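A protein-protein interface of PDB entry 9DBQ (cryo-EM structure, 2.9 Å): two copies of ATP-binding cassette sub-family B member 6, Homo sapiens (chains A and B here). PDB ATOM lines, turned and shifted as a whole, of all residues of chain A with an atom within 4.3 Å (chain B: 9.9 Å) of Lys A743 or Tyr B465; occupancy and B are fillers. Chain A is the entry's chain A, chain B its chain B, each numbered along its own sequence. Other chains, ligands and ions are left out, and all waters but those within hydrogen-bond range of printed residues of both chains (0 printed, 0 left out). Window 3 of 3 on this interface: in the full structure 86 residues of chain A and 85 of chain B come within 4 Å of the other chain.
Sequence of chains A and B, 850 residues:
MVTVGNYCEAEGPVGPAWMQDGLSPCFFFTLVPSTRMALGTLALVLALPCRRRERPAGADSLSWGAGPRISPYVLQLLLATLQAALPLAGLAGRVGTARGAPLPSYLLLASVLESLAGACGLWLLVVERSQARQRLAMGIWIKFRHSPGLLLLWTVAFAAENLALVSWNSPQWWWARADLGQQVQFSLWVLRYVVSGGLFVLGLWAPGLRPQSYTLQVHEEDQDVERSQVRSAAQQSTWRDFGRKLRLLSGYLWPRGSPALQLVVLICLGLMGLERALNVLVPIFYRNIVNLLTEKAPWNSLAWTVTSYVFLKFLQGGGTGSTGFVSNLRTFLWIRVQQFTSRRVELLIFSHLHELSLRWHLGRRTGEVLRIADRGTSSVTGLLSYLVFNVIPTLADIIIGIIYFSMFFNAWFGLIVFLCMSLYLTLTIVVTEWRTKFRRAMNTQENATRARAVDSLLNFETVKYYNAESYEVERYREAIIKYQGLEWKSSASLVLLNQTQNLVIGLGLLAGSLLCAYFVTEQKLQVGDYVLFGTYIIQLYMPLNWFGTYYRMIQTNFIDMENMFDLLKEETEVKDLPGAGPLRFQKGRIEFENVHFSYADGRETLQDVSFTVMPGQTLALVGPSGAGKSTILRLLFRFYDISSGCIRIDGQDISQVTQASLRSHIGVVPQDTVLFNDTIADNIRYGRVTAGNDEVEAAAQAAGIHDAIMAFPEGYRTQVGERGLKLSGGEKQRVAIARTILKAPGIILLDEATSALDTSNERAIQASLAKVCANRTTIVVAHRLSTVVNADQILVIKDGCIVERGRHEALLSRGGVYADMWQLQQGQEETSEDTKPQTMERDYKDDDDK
The backbone carbonyl oxygen (O) of Tyr B465 lies within hydrogen-bond range of the side-chain amino group (NZ) of Lys A743 (3.4 Å).
Among the printed residues, pairs that only touch across the chains: Phe A637 with Lys B464, Phe A637 with Tyr B465, Phe A639 with Lys B464, Phe A639 with Tyr B465, Val A668 with Tyr B465 and Arg A739 with Tyr B466.
Printed residues of chain B within 4 Å of Phe A637: Lys B464 and Tyr B465. Printed residues of chain B within 4 Å of Arg A739: Tyr B466 (3.7 Å). No residue of chain B comes within 4 Å of Leu A742. No residue of chain B comes within 4 Å of Ala A744. Val B463 touches none of the printed residues of chain A. Of the printed residues of chain A, Lys B464 touches Phe A637 (3.7 Å) and Phe A639 (3.7 Å). Printed residues of chain A within 4 Å of Tyr B465: Phe A637 (3.9 Å), Phe A639 (3.6 Å), Val A668 (3.5 Å) and Lys A743 (3.4 Å). The nearest residue of chain B that does not touch Lys A743 is Tyr B466 (4.4 Å). The nearest printed residue of chain B that does not touch Phe A637 is Tyr B466 (5.7 Å).
Printed residues of chain B that touch a printed residue of chain A: Lys B464, Tyr B465 and Tyr B466. Hydrophobic or aromatic side chains of chain B that line the printed part of chain A: Tyr B465 and Tyr B466. Hydrophobic or aromatic side chains of chain A within 4 Å of the printed part of chain B: Phe A637, Phe A639 and Val A668.
No position is printed for both chains.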
ATOM      1  N   PHE A 637     -30.333  -9.822   5.740  1.00  0.00           N
ATOM      2  CA  PHE A 637     -28.971  -9.399   6.034  1.00  0.00           C
ATOM      3  C   PHE A 637     -28.836  -7.885   6.059  1.00  0.00           C
ATOM      4  O   PHE A 637     -27.751  -7.379   6.363  1.00  0.00           O
ATOM      5  CB  PHE A 637     -28.017  -9.985   4.992  1.00  0.00           C
ATOM      6  CG  PHE A 637     -26.648 -10.298   5.517  1.00  0.00           C
ATOM      7  CD1 PHE A 637     -26.434 -11.419   6.296  1.00  0.00           C
ATOM      8  CD2 PHE A 637     -25.572  -9.488   5.205  1.00  0.00           C
ATOM      9  CE1 PHE A 637     -25.176 -11.719   6.770  1.00  0.00           C
ATOM     10  CE2 PHE A 637     -24.309  -9.781   5.674  1.00  0.00           C
ATOM     11  CZ  PHE A 637     -24.111 -10.901   6.457  1.00  0.00           C
ATOM     12  N   PHE A 639     -28.865  -5.807   3.542  1.00  0.00           N
ATOM     13  CA  PHE A 639     -28.261  -5.171   2.379  1.00  0.00           C
ATOM     14  C   PHE A 639     -29.137  -4.032   1.872  1.00  0.00           C
ATOM     15  O   PHE A 639     -28.631  -2.978   1.474  1.00  0.00           O
ATOM     16  CB  PHE A 639     -28.040  -6.194   1.269  1.00  0.00           C
ATOM     17  CG  PHE A 639     -26.881  -7.111   1.507  1.00  0.00           C
ATOM     18  CD1 PHE A 639     -25.584  -6.651   1.377  1.00  0.00           C
ATOM     19  CD2 PHE A 639     -27.086  -8.439   1.833  1.00  0.00           C
ATOM     20  CE1 PHE A 639     -24.509  -7.492   1.585  1.00  0.00           C
ATOM     21  CE2 PHE A 639     -26.017  -9.291   2.040  1.00  0.00           C
ATOM     22  CZ  PHE A 639     -24.724  -8.816   1.916  1.00  0.00           C
ATOM     23  N   SER A 664     -23.346 -10.249  12.615  1.00  0.00           N
ATOM     24  CA  SER A 664     -22.380 -11.207  13.142  1.00  0.00           C
ATOM     25  C   SER A 664     -23.017 -12.559  13.442  1.00  0.00           C
ATOM     26  O   SER A 664     -22.337 -13.589  13.372  1.00  0.00           O
ATOM     27  CB  SER A 664     -21.732 -10.641  14.403  1.00  0.00           C
ATOM     28  OG  SER A 664     -22.722 -10.172  15.302  1.00  0.00           O
ATOM     29  N   ILE A 666     -25.377 -14.095  11.778  1.00  0.00           N
ATOM     30  CA  ILE A 666     -25.971 -14.691  10.589  1.00  0.00           C
ATOM     31  C   ILE A 666     -24.861 -15.311   9.753  1.00  0.00           C
ATOM     32  O   ILE A 666     -23.875 -14.641   9.425  1.00  0.00           O
ATOM     33  CB  ILE A 666     -26.753 -13.655   9.761  1.00  0.00           C
ATOM     34  CG1 ILE A 666     -28.085 -13.316  10.432  1.00  0.00           C
ATOM     35  CG2 ILE A 666     -27.000 -14.172   8.358  1.00  0.00           C
ATOM     36  CD1 ILE A 666     -29.111 -14.420  10.363  1.00  0.00           C
ATOM     37  N   VAL A 668     -24.064 -17.321   6.121  1.00  0.00           N
ATOM     38  CA  VAL A 668     -24.587 -17.483   4.771  1.00  0.00           C
ATOM     39  C   VAL A 668     -23.685 -18.436   4.004  1.00  0.00           C
ATOM     40  O   VAL A 668     -22.458 -18.394   4.142  1.00  0.00           O
ATOM     41  CB  VAL A 668     -24.687 -16.138   4.029  1.00  0.00           C
ATOM     42  CG1 VAL A 668     -25.795 -15.288   4.616  1.00  0.00           C
ATOM     43  CG2 VAL A 668     -23.360 -15.405   4.085  1.00  0.00           C
ATOM     44  N   PRO A 670     -23.026 -18.954   0.242  1.00  0.00           N
ATOM     45  CA  PRO A 670     -23.407 -18.315  -1.021  1.00  0.00           C
ATOM     46  C   PRO A 670     -23.534 -19.325  -2.148  1.00  0.00           C
ATOM     47  O   PRO A 670     -23.159 -20.494  -2.037  1.00  0.00           O
ATOM     48  CB  PRO A 670     -22.264 -17.329  -1.274  1.00  0.00           C
ATOM     49  CG  PRO A 670     -21.109 -17.920  -0.585  1.00  0.00           C
ATOM     50  CD  PRO A 670     -21.654 -18.601   0.635  1.00  0.00           C
ATOM     51  N   GLY A 687     -13.219 -16.654   7.858  1.00  0.00           N
ATOM     52  CA  GLY A 687     -14.415 -16.576   8.673  1.00  0.00           C
ATOM     53  C   GLY A 687     -14.163 -16.024  10.056  1.00  0.00           C
ATOM     54  O   GLY A 687     -15.093 -15.517  10.692  1.00  0.00           O
ATOM     55  N   ARG A 739     -15.687 -22.310   6.754  1.00  0.00           N
ATOM     56  CA  ARG A 739     -15.757 -20.906   7.148  1.00  0.00           C
ATOM     57  C   ARG A 739     -16.900 -20.672   8.123  1.00  0.00           C
ATOM     58  O   ARG A 739     -16.705 -20.099   9.201  1.00  0.00           O
ATOM     59  CB  ARG A 739     -15.934 -20.028   5.912  1.00  0.00           C
ATOM     60  CG  ARG A 739     -14.692 -19.329   5.429  1.00  0.00           C
ATOM     61  CD  ARG A 739     -14.870 -18.884   3.997  1.00  0.00           C
ATOM     62  NE  ARG A 739     -13.770 -18.056   3.518  1.00  0.00           N
ATOM     63  CZ  ARG A 739     -13.542 -17.781   2.242  1.00  0.00           C
ATOM     64  NH1 ARG A 739     -14.310 -18.269   1.282  1.00  0.00           N
ATOM     65  NH2 ARG A 739     -12.513 -17.006   1.919  1.00  0.00           N
ATOM     66  N   THR A 740     -18.104 -21.123   7.767  1.00  0.00           N
ATOM     67  CA  THR A 740     -19.258 -20.924   8.632  1.00  0.00           C
ATOM     68  C   THR A 740     -19.214 -21.809   9.869  1.00  0.00           C
ATOM     69  O   THR A 740     -19.936 -21.536  10.833  1.00  0.00           O
ATOM     70  CB  THR A 740     -20.553 -21.183   7.856  1.00  0.00           C
ATOM     71  OG1 THR A 740     -21.673 -20.734   8.627  1.00  0.00           O
ATOM     72  CG2 THR A 740     -20.720 -22.660   7.551  1.00  0.00           C
ATOM     73  N   ILE A 741     -18.389 -22.859   9.864  1.00  0.00           N
ATOM     74  CA  ILE A 741     -18.217 -23.673  11.065  1.00  0.00           C
ATOM     75  C   ILE A 741     -17.477 -22.883  12.136  1.00  0.00           C
ATOM     76  O   ILE A 741     -17.869 -22.880  13.308  1.00  0.00           O
ATOM     77  CB  ILE A 741     -17.489 -24.986  10.727  1.00  0.00           C
ATOM     78  CG1 ILE A 741     -18.489 -26.018  10.200  1.00  0.00           C
ATOM     79  CG2 ILE A 741     -16.756 -25.513  11.959  1.00  0.00           C
ATOM     80  CD1 ILE A 741     -17.859 -27.263   9.610  1.00  0.00           C
ATOM     81  N   LEU A 742     -16.392 -22.211  11.755  1.00  0.00           N
ATOM     82  CA  LEU A 742     -15.647 -21.406  12.714  1.00  0.00           C
ATOM     83  C   LEU A 742     -16.213 -20.000  12.868  1.00  0.00           C
ATOM     84  O   LEU A 742     -15.755 -19.260  13.746  1.00  0.00           O
ATOM     85  CB  LEU A 742     -14.166 -21.345  12.320  1.00  0.00           C
ATOM     86  CG  LEU A 742     -13.776 -20.890  10.914  1.00  0.00           C
ATOM     87  CD1 LEU A 742     -13.648 -19.382  10.829  1.00  0.00           C
ATOM     88  CD2 LEU A 742     -12.476 -21.567  10.502  1.00  0.00           C
ATOM     89  N   LYS A 743     -17.190 -19.613  12.045  1.00  0.00           N
ATOM     90  CA  LYS A 743     -17.901 -18.364  12.290  1.00  0.00           C
ATOM     91  C   LYS A 743     -18.768 -18.467  13.535  1.00  0.00           C
ATOM     92  O   LYS A 743     -19.011 -17.459  14.207  1.00  0.00           O
ATOM     93  CB  LYS A 743     -18.757 -17.997  11.075  1.00  0.00           C
ATOM     94  CG  LYS A 743     -19.611 -16.733  11.231  1.00  0.00           C
ATOM     95  CD  LYS A 743     -18.778 -15.466  11.133  1.00  0.00           C
ATOM     96  CE  LYS A 743     -19.651 -14.231  10.980  1.00  0.00           C
ATOM     97  NZ  LYS A 743     -20.409 -14.223   9.701  1.00  0.00           N
ATOM     98  N   ALA A 744     -19.233 -19.669  13.856  1.00  0.00           N
ATOM     99  CA  ALA A 744     -20.093 -19.894  15.010  1.00  0.00           C
ATOM    100  C   ALA A 744     -21.310 -18.978  14.956  1.00  0.00           C
ATOM    101  O   ALA A 744     -21.432 -18.058  15.774  1.00  0.00           O
ATOM    102  CB  ALA A 744     -19.315 -19.664  16.305  1.00  0.00           C
ATOM    103  N   PRO A 745     -22.222 -19.193  14.014  1.00  0.00           N
ATOM    104  CA  PRO A 745     -23.418 -18.357  13.916  1.00  0.00           C
ATOM    105  C   PRO A 745     -24.550 -18.896  14.784  1.00  0.00           C
ATOM    106  O   PRO A 745     -24.495 -20.008  15.310  1.00  0.00           O
ATOM    107  CB  PRO A 745     -23.769 -18.456  12.428  1.00  0.00           C
ATOM    108  CG  PRO A 745     -23.348 -19.823  12.055  1.00  0.00           C
ATOM    109  CD  PRO A 745     -22.146 -20.162  12.908  1.00  0.00           C
ATOM    110  N   ASN B 459     -15.023  -8.282  -4.706  1.00  0.00           N
ATOM    111  CA  ASN B 459     -15.775  -9.277  -3.943  1.00  0.00           C
ATOM    112  C   ASN B 459     -16.442  -8.622  -2.733  1.00  0.00           C
ATOM    113  O   ASN B 459     -16.275  -9.031  -1.586  1.00  0.00           O
ATOM    114  CB  ASN B 459     -14.858 -10.417  -3.521  1.00  0.00           C
ATOM    115  CG  ASN B 459     -14.086 -11.001  -4.684  1.00  0.00           C
ATOM    116  OD1 ASN B 459     -14.464 -10.831  -5.842  1.00  0.00           O
ATOM    117  ND2 ASN B 459     -12.999 -11.698  -4.381  1.00  0.00           N
ATOM    118  N   PHE B 460     -17.235  -7.590  -3.024  1.00  0.00           N
ATOM    119  CA  PHE B 460     -17.825  -6.787  -1.959  1.00  0.00           C
ATOM    120  C   PHE B 460     -18.783  -7.606  -1.105  1.00  0.00           C
ATOM    121  O   PHE B 460     -18.841  -7.428   0.115  1.00  0.00           O
ATOM    122  CB  PHE B 460     -18.546  -5.580  -2.557  1.00  0.00           C
ATOM    123  CG  PHE B 460     -19.157  -4.678  -1.533  1.00  0.00           C
ATOM    124  CD1 PHE B 460     -18.358  -3.891  -0.728  1.00  0.00           C
ATOM    125  CD2 PHE B 460     -20.531  -4.610  -1.381  1.00  0.00           C
ATOM    126  CE1 PHE B 460     -18.913  -3.056   0.218  1.00  0.00           C
ATOM    127  CE2 PHE B 460     -21.098  -3.777  -0.436  1.00  0.00           C
ATOM    128  CZ  PHE B 460     -20.286  -2.995   0.366  1.00  0.00           C
ATOM    129  N   GLU B 461     -19.550  -8.502  -1.724  1.00  0.00           N
ATOM    130  CA  GLU B 461     -20.550  -9.251  -0.972  1.00  0.00           C
ATOM    131  C   GLU B 461     -19.905 -10.145   0.080  1.00  0.00           C
ATOM    132  O   GLU B 461     -20.403 -10.240   1.206  1.00  0.00           O
ATOM    133  CB  GLU B 461     -21.406 -10.077  -1.926  1.00  0.00           C
ATOM    134  CG  GLU B 461     -22.302  -9.238  -2.821  1.00  0.00           C
ATOM    135  CD  GLU B 461     -23.030 -10.069  -3.858  1.00  0.00           C
ATOM    136  OE1 GLU B 461     -22.681 -11.254  -4.029  1.00  0.00           O
ATOM    137  OE2 GLU B 461     -23.956  -9.535  -4.506  1.00  0.00           O
ATOM    138  N   THR B 462     -18.806 -10.818  -0.267  1.00  0.00           N
ATOM    139  CA  THR B 462     -18.152 -11.696   0.701  1.00  0.00           C
ATOM    140  C   THR B 462     -17.528 -10.899   1.837  1.00  0.00           C
ATOM    141  O   THR B 462     -17.560 -11.330   2.994  1.00  0.00           O
ATOM    142  CB  THR B 462     -17.092 -12.549   0.013  1.00  0.00           C
ATOM    143  OG1 THR B 462     -16.179 -11.700  -0.689  1.00  0.00           O
ATOM    144  CG2 THR B 462     -17.740 -13.520  -0.958  1.00  0.00           C
ATOM    145  N   VAL B 463     -16.953  -9.735   1.531  1.00  0.00           N
ATOM    146  CA  VAL B 463     -16.378  -8.897   2.578  1.00  0.00           C
ATOM    147  C   VAL B 463     -17.445  -8.509   3.587  1.00  0.00           C
ATOM    148  O   VAL B 463     -17.238  -8.604   4.801  1.00  0.00           O
ATOM    149  CB  VAL B 463     -15.711  -7.658   1.957  1.00  0.00           C
ATOM    150  CG1 VAL B 463     -15.273  -6.693   3.038  1.00  0.00           C
ATOM    151  CG2 VAL B 463     -14.535  -8.066   1.099  1.00  0.00           C
ATOM    152  N   LYS B 464     -18.612  -8.083   3.104  1.00  0.00           N
ATOM    153  CA  LYS B 464     -19.707  -7.767   4.011  1.00  0.00           C
ATOM    154  C   LYS B 464     -20.220  -9.012   4.719  1.00  0.00           C
ATOM    155  O   LYS B 464     -20.749  -8.915   5.828  1.00  0.00           O
ATOM    156  CB  LYS B 464     -20.846  -7.089   3.251  1.00  0.00           C
ATOM    157  CG  LYS B 464     -20.789  -5.569   3.264  1.00  0.00           C
ATOM    158  CD  LYS B 464     -22.092  -4.951   2.775  1.00  0.00           C
ATOM    159  CE  LYS B 464     -22.211  -3.491   3.194  1.00  0.00           C
ATOM    160  NZ  LYS B 464     -23.496  -2.870   2.755  1.00  0.00           N
ATOM    161  N   TYR B 465     -20.074 -10.187   4.105  1.00  0.00           N
ATOM    162  CA  TYR B 465     -20.560 -11.408   4.738  1.00  0.00           C
ATOM    163  C   TYR B 465     -19.791 -11.712   6.016  1.00  0.00           C
ATOM    164  O   TYR B 465     -20.388 -12.009   7.056  1.00  0.00           O
ATOM    165  CB  TYR B 465     -20.451 -12.588   3.771  1.00  0.00           C
ATOM    166  CG  TYR B 465     -21.540 -12.692   2.725  1.00  0.00           C
ATOM    167  CD1 TYR B 465     -22.795 -12.135   2.923  1.00  0.00           C
ATOM    168  CD2 TYR B 465     -21.307 -13.368   1.539  1.00  0.00           C
ATOM    169  CE1 TYR B 465     -23.783 -12.249   1.963  1.00  0.00           C
ATOM    170  CE2 TYR B 465     -22.285 -13.482   0.577  1.00  0.00           C
ATOM    171  CZ  TYR B 465     -23.519 -12.924   0.792  1.00  0.00           C
ATOM    172  OH  TYR B 465     -24.493 -13.041  -0.175  1.00  0.00           O
ATOM    173  N   TYR B 466     -18.462 -11.647   5.957  1.00  0.00           N
ATOM    174  CA  TYR B 466     -17.608 -12.119   7.041  1.00  0.00           C
ATOM    175  C   TYR B 466     -17.070 -10.993   7.914  1.00  0.00           C
ATOM    176  O   TYR B 466     -16.284 -11.260   8.825  1.00  0.00           O
ATOM    177  CB  TYR B 466     -16.452 -12.944   6.468  1.00  0.00           C
ATOM    178  CG  TYR B 466     -16.928 -14.162   5.721  1.00  0.00           C
ATOM    179  CD1 TYR B 466     -17.597 -15.179   6.381  1.00  0.00           C
ATOM    180  CD2 TYR B 466     -16.724 -14.287   4.358  1.00  0.00           C
ATOM    181  CE1 TYR B 466     -18.045 -16.287   5.704  1.00  0.00           C
ATOM    182  CE2 TYR B 466     -17.168 -15.394   3.674  1.00  0.00           C
ATOM    183  CZ  TYR B 466     -17.830 -16.390   4.350  1.00  0.00           C
ATOM    184  OH  TYR B 466     -18.275 -17.497   3.666  1.00  0.00           O
ATOM    185  N   ASN B 467     -17.482  -9.749   7.673  1.00  0.00           N
ATOM    186  CA  ASN B 467     -17.081  -8.613   8.500  1.00  0.00           C
ATOM    187  C   ASN B 467     -15.560  -8.451   8.506  1.00  0.00           C
ATOM    188  O   ASN B 467     -14.893  -8.604   9.530  1.00  0.00           O
ATOM    189  CB  ASN B 467     -17.619  -8.764   9.928  1.00  0.00           C
ATOM    190  CG  ASN B 467     -19.020  -8.219  10.085  1.00  0.00           C
ATOM    191  OD1 ASN B 467     -19.429  -7.311   9.366  1.00  0.00           O
ATOM    192  ND2 ASN B 467     -19.761  -8.767  11.038  1.00  0.00           N
ATOM    193  N   ALA B 468     -15.017  -8.131   7.337  1.00  0.00           N
ATOM    194  CA  ALA B 468     -13.577  -8.007   7.158  1.00  0.00           C
ATOM    195  C   ALA B 468     -13.221  -6.700   6.467  1.00  0.00           C
ATOM    196  O   ALA B 468     -12.387  -6.666   5.559  1.00  0.00           O
ATOM    197  CB  ALA B 468     -13.029  -9.195   6.371  1.00  0.00           C
ATOM    198  N   GLU B 469     -13.860  -5.602   6.873  1.00  0.00           N
ATOM    199  CA  GLU B 469     -13.453  -4.294   6.372  1.00  0.00           C
ATOM    200  C   GLU B 469     -12.166  -3.825   7.037  1.00  0.00           C
ATOM    201  O   GLU B 469     -11.263  -3.314   6.370  1.00  0.00           O
ATOM    202  CB  GLU B 469     -14.568  -3.273   6.589  1.00  0.00           C
ATOM    203  CG  GLU B 469     -15.818  -3.539   5.765  1.00  0.00           C
ATOM    204  CD  GLU B 469     -16.898  -4.287   6.529  1.00  0.00           C
ATOM    205  OE1 GLU B 469     -16.731  -4.541   7.737  1.00  0.00           O
ATOM    206  OE2 GLU B 469     -17.929  -4.618   5.910  1.00  0.00           O
ATOM    207  N   GLU B 472      -9.226  -5.971   5.730  1.00  0.00           N
ATOM    208  CA  GLU B 472      -8.769  -5.697   4.373  1.00  0.00           C
ATOM    209  C   GLU B 472      -8.072  -4.348   4.256  1.00  0.00           C
ATOM    210  O   GLU B 472      -7.155  -4.204   3.442  1.00  0.00           O
ATOM    211  CB  GLU B 472      -9.937  -5.779   3.401  1.00  0.00           C
ATOM    212  CG  GLU B 472     -10.354  -7.208   3.122  1.00  0.00           C
ATOM    213  CD  GLU B 472     -11.126  -7.351   1.831  1.00  0.00           C
ATOM    214  OE1 GLU B 472     -11.714  -6.354   1.370  1.00  0.00           O
ATOM    215  OE2 GLU B 472     -11.138  -8.467   1.271  1.00  0.00           O
